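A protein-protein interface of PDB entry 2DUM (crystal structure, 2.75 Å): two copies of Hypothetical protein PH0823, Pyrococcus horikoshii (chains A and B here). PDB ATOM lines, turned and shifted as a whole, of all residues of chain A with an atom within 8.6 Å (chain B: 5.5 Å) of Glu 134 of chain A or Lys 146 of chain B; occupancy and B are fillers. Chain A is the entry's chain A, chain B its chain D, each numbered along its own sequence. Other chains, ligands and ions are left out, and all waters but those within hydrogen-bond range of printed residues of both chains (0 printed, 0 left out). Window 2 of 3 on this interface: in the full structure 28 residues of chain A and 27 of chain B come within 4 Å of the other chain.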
ATOM      1  N   SER A 125       9.788  25.915 -18.146  1.00  0.00           N
ATOM      2  CA  SER A 125       8.450  25.919 -18.754  1.00  0.00           C
ATOM      3  C   SER A 125       8.107  24.467 -18.987  1.00  0.00           C
ATOM      4  O   SER A 125       7.284  23.902 -18.262  1.00  0.00           O
ATOM      5  CB  SER A 125       8.313  26.782 -19.993  1.00  0.00           C
ATOM      6  OG  SER A 125       8.377  26.019 -21.183  1.00  0.00           O
ATOM      7  N   ARG A 126       8.769  23.809 -19.917  1.00  0.00           N
ATOM      8  CA  ARG A 126       8.433  22.413 -20.135  1.00  0.00           C
ATOM      9  C   ARG A 126       9.590  21.521 -19.711  1.00  0.00           C
ATOM     10  O   ARG A 126      10.796  21.885 -19.871  1.00  0.00           O
ATOM     11  CB  ARG A 126       7.904  22.135 -21.565  1.00  0.00           C
ATOM     12  CG  ARG A 126       8.479  22.999 -22.773  1.00  0.00           C
ATOM     13  CD  ARG A 126       9.471  22.156 -23.573  1.00  0.00           C
ATOM     14  NE  ARG A 126      10.137  22.837 -24.693  1.00  0.00           N
ATOM     15  CZ  ARG A 126      10.935  22.233 -25.615  1.00  0.00           C
ATOM     16  NH1 ARG A 126      11.499  22.961 -26.618  1.00  0.00           N
ATOM     17  NH2 ARG A 126      11.175  20.900 -25.569  1.00  0.00           N
ATOM     18  N   LEU A 131       9.773  19.106 -27.493  1.00  0.00           N
ATOM     19  CA  LEU A 131       8.942  19.811 -28.520  1.00  0.00           C
ATOM     20  C   LEU A 131       8.358  21.159 -28.037  1.00  0.00           C
ATOM     21  O   LEU A 131       7.374  21.175 -27.271  1.00  0.00           O
ATOM     22  CB  LEU A 131       7.797  18.893 -29.110  1.00  0.00           C
ATOM     23  CG  LEU A 131       6.779  19.259 -30.274  1.00  0.00           C
ATOM     24  CD1 LEU A 131       6.507  18.123 -31.319  1.00  0.00           C
ATOM     25  CD2 LEU A 131       5.432  19.862 -29.779  1.00  0.00           C
ATOM     26  N   SER A 132       8.980  22.262 -28.503  1.00  0.00           N
ATOM     27  CA  SER A 132       8.392  23.672 -28.616  1.00  0.00           C
ATOM     28  C   SER A 132       7.953  24.527 -27.360  1.00  0.00           C
ATOM     29  O   SER A 132       7.535  23.996 -26.283  1.00  0.00           O
ATOM     30  CB  SER A 132       7.335  23.805 -29.773  1.00  0.00           C
ATOM     31  OG  SER A 132       7.508  25.021 -30.520  1.00  0.00           O
ATOM     32  N   HIS A 133       8.034  25.858 -27.567  1.00  0.00           N
ATOM     33  CA  HIS A 133       7.890  26.880 -26.516  1.00  0.00           C
ATOM     34  C   HIS A 133       6.413  27.222 -26.169  1.00  0.00           C
ATOM     35  O   HIS A 133       6.131  28.369 -25.802  1.00  0.00           O
ATOM     36  CB  HIS A 133       8.673  28.155 -26.919  1.00  0.00           C
ATOM     37  CG  HIS A 133       7.861  29.133 -27.723  1.00  0.00           C
ATOM     38  ND1 HIS A 133       6.953  28.743 -28.691  1.00  0.00           N
ATOM     39  CD2 HIS A 133       7.803  30.485 -27.688  1.00  0.00           C
ATOM     40  CE1 HIS A 133       6.386  29.811 -29.223  1.00  0.00           C
ATOM     41  NE2 HIS A 133       6.885  30.883 -28.633  1.00  0.00           N
ATOM     42  N   GLU A 134       5.485  26.257 -26.287  1.00  0.00           N
ATOM     43  CA  GLU A 134       4.077  26.511 -25.943  1.00  0.00           C
ATOM     44  C   GLU A 134       3.483  25.481 -25.033  1.00  0.00           C
ATOM     45  O   GLU A 134       2.599  25.796 -24.209  1.00  0.00           O
ATOM     46  CB  GLU A 134       3.199  26.716 -27.177  1.00  0.00           C
ATOM     47  CG  GLU A 134       3.324  28.133 -27.736  1.00  0.00           C
ATOM     48  CD  GLU A 134       2.223  28.502 -28.685  1.00  0.00           C
ATOM     49  OE1 GLU A 134       2.497  29.313 -29.613  1.00  0.00           O
ATOM     50  OE2 GLU A 134       1.095  27.979 -28.482  1.00  0.00           O
ATOM     51  N   PHE A 135       3.943  24.237 -25.178  1.00  0.00           N
ATOM     52  CA  PHE A 135       3.481  23.232 -24.223  1.00  0.00           C
ATOM     53  C   PHE A 135       3.932  23.818 -22.879  1.00  0.00           C
ATOM     54  O   PHE A 135       5.157  24.030 -22.656  1.00  0.00           O
ATOM     55  CB  PHE A 135       3.932  21.732 -24.458  1.00  0.00           C
ATOM     56  CG  PHE A 135       3.503  20.776 -23.294  1.00  0.00           C
ATOM     57  CD1 PHE A 135       2.129  20.664 -22.898  1.00  0.00           C
ATOM     58  CD2 PHE A 135       4.458  20.064 -22.534  1.00  0.00           C
ATOM     59  CE1 PHE A 135       1.710  19.835 -21.764  1.00  0.00           C
ATOM     60  CE2 PHE A 135       4.048  19.228 -21.400  1.00  0.00           C
ATOM     61  CZ  PHE A 135       2.684  19.112 -21.034  1.00  0.00           C
ATOM     62  N   LEU A 136       2.953  24.143 -22.029  1.00  0.00           N
ATOM     63  CA  LEU A 136       3.300  24.693 -20.766  1.00  0.00           C
ATOM     64  C   LEU A 136       3.895  23.725 -19.766  1.00  0.00           C
ATOM     65  O   LEU A 136       4.900  24.007 -19.172  1.00  0.00           O
ATOM     66  CB  LEU A 136       2.172  25.472 -20.156  1.00  0.00           C
ATOM     67  CG  LEU A 136       3.020  26.532 -19.457  1.00  0.00           C
ATOM     68  CD1 LEU A 136       4.052  27.241 -20.465  1.00  0.00           C
ATOM     69  CD2 LEU A 136       2.174  27.488 -18.559  1.00  0.00           C
ATOM     70  N   GLY A 137       3.329  22.572 -19.546  1.00  0.00           N
ATOM     71  CA  GLY A 137       3.793  21.844 -18.378  1.00  0.00           C
ATOM     72  C   GLY A 137       2.645  22.038 -17.438  1.00  0.00           C
ATOM     73  O   GLY A 137       2.063  23.121 -17.366  1.00  0.00           O
ATOM     74  N   MET A 141       1.908  25.041 -14.446  1.00  0.00           N
ATOM     75  CA  MET A 141       0.557  25.427 -14.227  1.00  0.00           C
ATOM     76  C   MET A 141       0.001  25.237 -12.778  1.00  0.00           C
ATOM     77  O   MET A 141      -0.659  26.149 -12.205  1.00  0.00           O
ATOM     78  CB  MET A 141      -0.312  24.629 -15.179  1.00  0.00           C
ATOM     79  CG  MET A 141      -0.288  25.083 -16.620  1.00  0.00           C
ATOM     80  SD  MET A 141      -0.554  26.871 -16.839  1.00  0.00           S
ATOM     81  CE  MET A 141      -0.914  26.863 -18.635  1.00  0.00           C
ATOM     82  N   LYS A 155      12.562  29.562 -19.902  1.00  0.00           N
ATOM     83  CA  LYS A 155      12.161  28.824 -21.088  1.00  0.00           C
ATOM     84  C   LYS A 155      13.262  28.437 -22.111  1.00  0.00           C
ATOM     85  O   LYS A 155      13.426  27.244 -22.444  1.00  0.00           O
ATOM     86  CB  LYS A 155      11.072  29.625 -21.774  1.00  0.00           C
ATOM     87  CG  LYS A 155       9.906  28.805 -22.288  1.00  0.00           C
ATOM     88  CD  LYS A 155       8.827  29.670 -22.887  1.00  0.00           C
ATOM     89  CE  LYS A 155       7.830  30.183 -21.865  1.00  0.00           C
ATOM     90  NZ  LYS A 155       6.502  30.268 -22.606  1.00  0.00           N
ATOM     91  N   TRP B 106      -2.298  40.519 -24.742  1.00  0.00           N
ATOM     92  CA  TRP B 106      -1.194  39.518 -24.842  1.00  0.00           C
ATOM     93  C   TRP B 106      -0.580  39.547 -26.236  1.00  0.00           C
ATOM     94  O   TRP B 106       0.540  39.221 -26.411  1.00  0.00           O
ATOM     95  CB  TRP B 106      -1.638  38.103 -24.498  1.00  0.00           C
ATOM     96  CG  TRP B 106      -2.657  37.654 -25.525  1.00  0.00           C
ATOM     97  CD1 TRP B 106      -4.045  37.723 -25.403  1.00  0.00           C
ATOM     98  CD2 TRP B 106      -2.385  37.170 -26.862  1.00  0.00           C
ATOM     99  NE1 TRP B 106      -4.614  37.292 -26.569  1.00  0.00           N
ATOM    100  CE2 TRP B 106      -3.631  36.942 -27.476  1.00  0.00           C
ATOM    101  CE3 TRP B 106      -1.205  36.875 -27.574  1.00  0.00           C
ATOM    102  CZ2 TRP B 106      -3.745  36.455 -28.793  1.00  0.00           C
ATOM    103  CZ3 TRP B 106      -1.298  36.373 -28.859  1.00  0.00           C
ATOM    104  CH2 TRP B 106      -2.581  36.187 -29.471  1.00  0.00           C
ATOM    105  N   VAL B 110       3.601  40.452 -26.184  1.00  0.00           N
ATOM    106  CA  VAL B 110       4.651  39.541 -26.572  1.00  0.00           C
ATOM    107  C   VAL B 110       5.473  40.320 -27.594  1.00  0.00           C
ATOM    108  O   VAL B 110       6.725  40.255 -27.670  1.00  0.00           O
ATOM    109  CB  VAL B 110       4.098  38.295 -27.167  1.00  0.00           C
ATOM    110  CG1 VAL B 110       5.193  37.610 -27.962  1.00  0.00           C
ATOM    111  CG2 VAL B 110       3.423  37.318 -26.085  1.00  0.00           C
ATOM    112  N   GLU B 114       9.503  41.163 -27.527  1.00  0.00           N
ATOM    113  CA  GLU B 114      10.462  40.818 -28.553  1.00  0.00           C
ATOM    114  C   GLU B 114      10.987  42.149 -29.038  1.00  0.00           C
ATOM    115  O   GLU B 114      12.154  42.396 -28.923  1.00  0.00           O
ATOM    116  CB  GLU B 114       9.918  40.007 -29.715  1.00  0.00           C
ATOM    117  CG  GLU B 114       9.020  38.804 -29.369  1.00  0.00           C
ATOM    118  CD  GLU B 114       9.645  37.719 -28.381  1.00  0.00           C
ATOM    119  OE1 GLU B 114      10.879  37.470 -28.511  1.00  0.00           O
ATOM    120  OE2 GLU B 114       8.893  37.107 -27.491  1.00  0.00           O
ATOM    121  N   ARG B 142      -2.015  33.783 -21.485  1.00  0.00           N
ATOM    122  CA  ARG B 142      -1.733  33.625 -22.887  1.00  0.00           C
ATOM    123  C   ARG B 142      -0.379  34.032 -23.318  1.00  0.00           C
ATOM    124  O   ARG B 142       0.156  33.399 -24.254  1.00  0.00           O
ATOM    125  CB  ARG B 142      -2.674  34.425 -23.753  1.00  0.00           C
ATOM    126  CG  ARG B 142      -2.283  34.302 -25.269  1.00  0.00           C
ATOM    127  CD  ARG B 142      -2.741  32.990 -25.878  1.00  0.00           C
ATOM    128  NE  ARG B 142      -4.153  32.792 -25.484  1.00  0.00           N
ATOM    129  CZ  ARG B 142      -5.205  33.043 -26.264  1.00  0.00           C
ATOM    130  NH1 ARG B 142      -6.426  32.846 -25.807  1.00  0.00           N
ATOM    131  NH2 ARG B 142      -5.018  33.441 -27.529  1.00  0.00           N
ATOM    132  N   VAL B 143       0.114  35.151 -22.737  1.00  0.00           N
ATOM    133  CA  VAL B 143       1.456  35.740 -23.020  1.00  0.00           C
ATOM    134  C   VAL B 143       2.390  34.670 -22.609  1.00  0.00           C
ATOM    135  O   VAL B 143       3.456  34.444 -23.245  1.00  0.00           O
ATOM    136  CB  VAL B 143       1.815  36.974 -22.110  1.00  0.00           C
ATOM    137  CG1 VAL B 143       1.366  38.272 -22.674  1.00  0.00           C
ATOM    138  CG2 VAL B 143       1.115  36.878 -20.920  1.00  0.00           C
ATOM    139  N   LEU B 144       1.938  33.995 -21.541  1.00  0.00           N
ATOM    140  CA  LEU B 144       2.663  32.981 -20.834  1.00  0.00           C
ATOM    141  C   LEU B 144       2.899  31.708 -21.612  1.00  0.00           C
ATOM    142  O   LEU B 144       3.153  30.677 -21.045  1.00  0.00           O
ATOM    143  CB  LEU B 144       1.898  32.605 -19.592  1.00  0.00           C
ATOM    144  CG  LEU B 144       2.779  32.481 -18.374  1.00  0.00           C
ATOM    145  CD1 LEU B 144       2.328  31.320 -17.556  1.00  0.00           C
ATOM    146  CD2 LEU B 144       4.256  32.334 -18.732  1.00  0.00           C
ATOM    147  N   ARG B 145       2.824  31.762 -22.917  1.00  0.00           N
ATOM    148  CA  ARG B 145       2.737  30.560 -23.660  1.00  0.00           C
ATOM    149  C   ARG B 145       3.037  31.077 -25.029  1.00  0.00           C
ATOM    150  O   ARG B 145       3.704  30.409 -25.810  1.00  0.00           O
ATOM    151  CB  ARG B 145       1.302  30.021 -23.541  1.00  0.00           C
ATOM    152  CG  ARG B 145       1.041  28.548 -23.933  1.00  0.00           C
ATOM    153  CD  ARG B 145       0.519  28.383 -25.397  1.00  0.00           C
ATOM    154  NE  ARG B 145      -0.949  28.537 -25.560  1.00  0.00           N
ATOM    155  CZ  ARG B 145      -1.546  28.779 -26.733  1.00  0.00           C
ATOM    156  NH1 ARG B 145      -0.840  28.916 -27.849  1.00  0.00           N
ATOM    157  NH2 ARG B 145      -2.843  28.913 -26.798  1.00  0.00           N
ATOM    158  N   LYS B 146       2.598  32.282 -25.332  1.00  0.00           N
ATOM    159  CA  LYS B 146       3.017  32.763 -26.580  1.00  0.00           C
ATOM    160  C   LYS B 146       4.442  33.353 -26.630  1.00  0.00           C
ATOM    161  O   LYS B 146       4.989  33.552 -27.737  1.00  0.00           O
ATOM    162  CB  LYS B 146       1.969  33.672 -27.176  1.00  0.00           C
ATOM    163  CG  LYS B 146       0.951  32.947 -28.025  1.00  0.00           C
ATOM    164  CD  LYS B 146       1.578  32.446 -29.388  1.00  0.00           C
ATOM    165  CE  LYS B 146       0.531  31.731 -30.335  1.00  0.00           C
ATOM    166  NZ  LYS B 146      -0.213  30.609 -29.652  1.00  0.00           N
ATOM    167  N   THR B 147       5.055  33.628 -25.467  1.00  0.00           N
ATOM    168  CA  THR B 147       6.354  34.344 -25.465  1.00  0.00           C
ATOM    169  C   THR B 147       7.621  33.555 -25.278  1.00  0.00           C
ATOM    170  O   THR B 147       7.731  32.623 -24.495  1.00  0.00           O
ATOM    171  CB  THR B 147       6.477  35.465 -24.457  1.00  0.00           C
ATOM    172  OG1 THR B 147       7.470  36.377 -24.975  1.00  0.00           O
ATOM    173  CG2 THR B 147       6.934  34.941 -23.149  1.00  0.00           C
ATOM    174  N   LYS B 148       8.637  34.014 -25.969  1.00  0.00           N
ATOM    175  CA  LYS B 148       9.937  33.378 -25.791  1.00  0.00           C
ATOM    176  C   LYS B 148      10.790  33.879 -24.536  1.00  0.00           C
ATOM    177  O   LYS B 148      11.655  33.127 -23.984  1.00  0.00           O
ATOM    178  CB  LYS B 148      10.630  33.353 -27.147  1.00  0.00           C
ATOM    179  CG  LYS B 148      10.138  32.070 -27.980  1.00  0.00           C
ATOM    180  CD  LYS B 148       9.721  32.236 -29.503  1.00  0.00           C
ATOM    181  CE  LYS B 148      10.917  32.591 -30.419  1.00  0.00           C
ATOM    182  NZ  LYS B 148      11.776  33.867 -30.141  1.00  0.00           N
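Of chain B, only Arg 145 and Lys 146 come within 4 Å of Glu 134 of chain A. Printed residues of chain B within 4 Å of Leu 136 of chain A: Leu 144 (3.6 Å). Of the printed residues of chain B, Lys 155 of chain A touches Leu 144, Arg 145 and Thr 147. Of the printed residues of chain A, Leu 144 of chain B touches Leu 136 and Lys 155. Of chain A, only His 133 and Glu 134 come within 4 Å of Lys 146 of chain B. Of the printed residues of chain A, Thr 147 of chain B touches His 133 (3.8 Å) and Lys 155 (3.3 Å). Printed residues of chain A within 4 Å of Lys 148 of chain B: His 133 (2.8 Å). The nearest printed residue of chain B that does not touch Glu 134 of chain A is Leu 144 of chain B (5.8 Å). The nearest residue of chain A that does not touch Lys 146 of chain B is Lys 155 of chain A (5.2 Å). The nearest printed residue of chain B that does not touch Leu 136 of chain A is Arg 145 of chain B (4.8 Å).
No position is printed for both chains.
O of Arg 145 of chain B sits close to O of His 133 of chain A (3.2 Å). The side-chain carboxylate of Glu 134 of chain A lies within salt-bridge range of the side-chain amino group of Lys 146 of chain B, at 3.0 Å. The backbone carbonyl oxygen of Thr 147 of chain B sits at hydrogen-bond distance from the side-chain amino group of Lys 155 of chain A (3.3 Å). NE of Arg 145 of chain B is in salt-bridge range of OE2 of Glu 134 of chain A, at 3.6 Å. NE2 of His 133 of chain A sits at hydrogen-bond distance from O of Lys 146 of chain B.
The backbone carbonyl oxygen (O) of Leu 136 of chain A lies close to the backbone carbonyl oxygen (O) of Ser 125 of chain A (2.6 Å). The backbone NH (N) of Lys 148 of chain B is in hydrogen-bond range of the side-chain carboxylate (OE2) of Glu 114 of chain B. The side-chain amino group (NZ) of Lys 146 of chain B lies close to the guanidinium group (NH1) of Arg 145 of chain B, at 2.6 Å. The side-chain carboxylate of Glu 114 of chain B is in hydrogen-bond range of the side-chain hydroxyl of Thr 147 of chain B, at 3.0 Å.
Hydrophobic or aromatic side chains of chain A within 4 Å of the printed part of chain B: His 133 and Leu 136. Hydrophobic or aromatic side chains of chain B within 4 Å of the printed part of chain A: Leu 144. Among the printed residues, 10 pairs touch across the chains. Among the printed residues, Asp or Glu carboxylates within 4 Å of a Lys or Arg side-chain nitrogen of the other chain: Glu 134 of chain A with Arg 145 of chain B (2.2 Å) and Glu 134 of chain A with Lys 146 of chain B (3.0 Å).
Among the printed residues, pairs that only touch across the chains: His 133 of chain A with Thr 147 of chain B, His 133 of chain A with Lys 148 of chain B, Leu 136 of chain A with Leu 144 of chain B, Lys 155 of chain A with Leu 144 of chain B and Lys 155 of chain A with Arg 145 of chain B.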
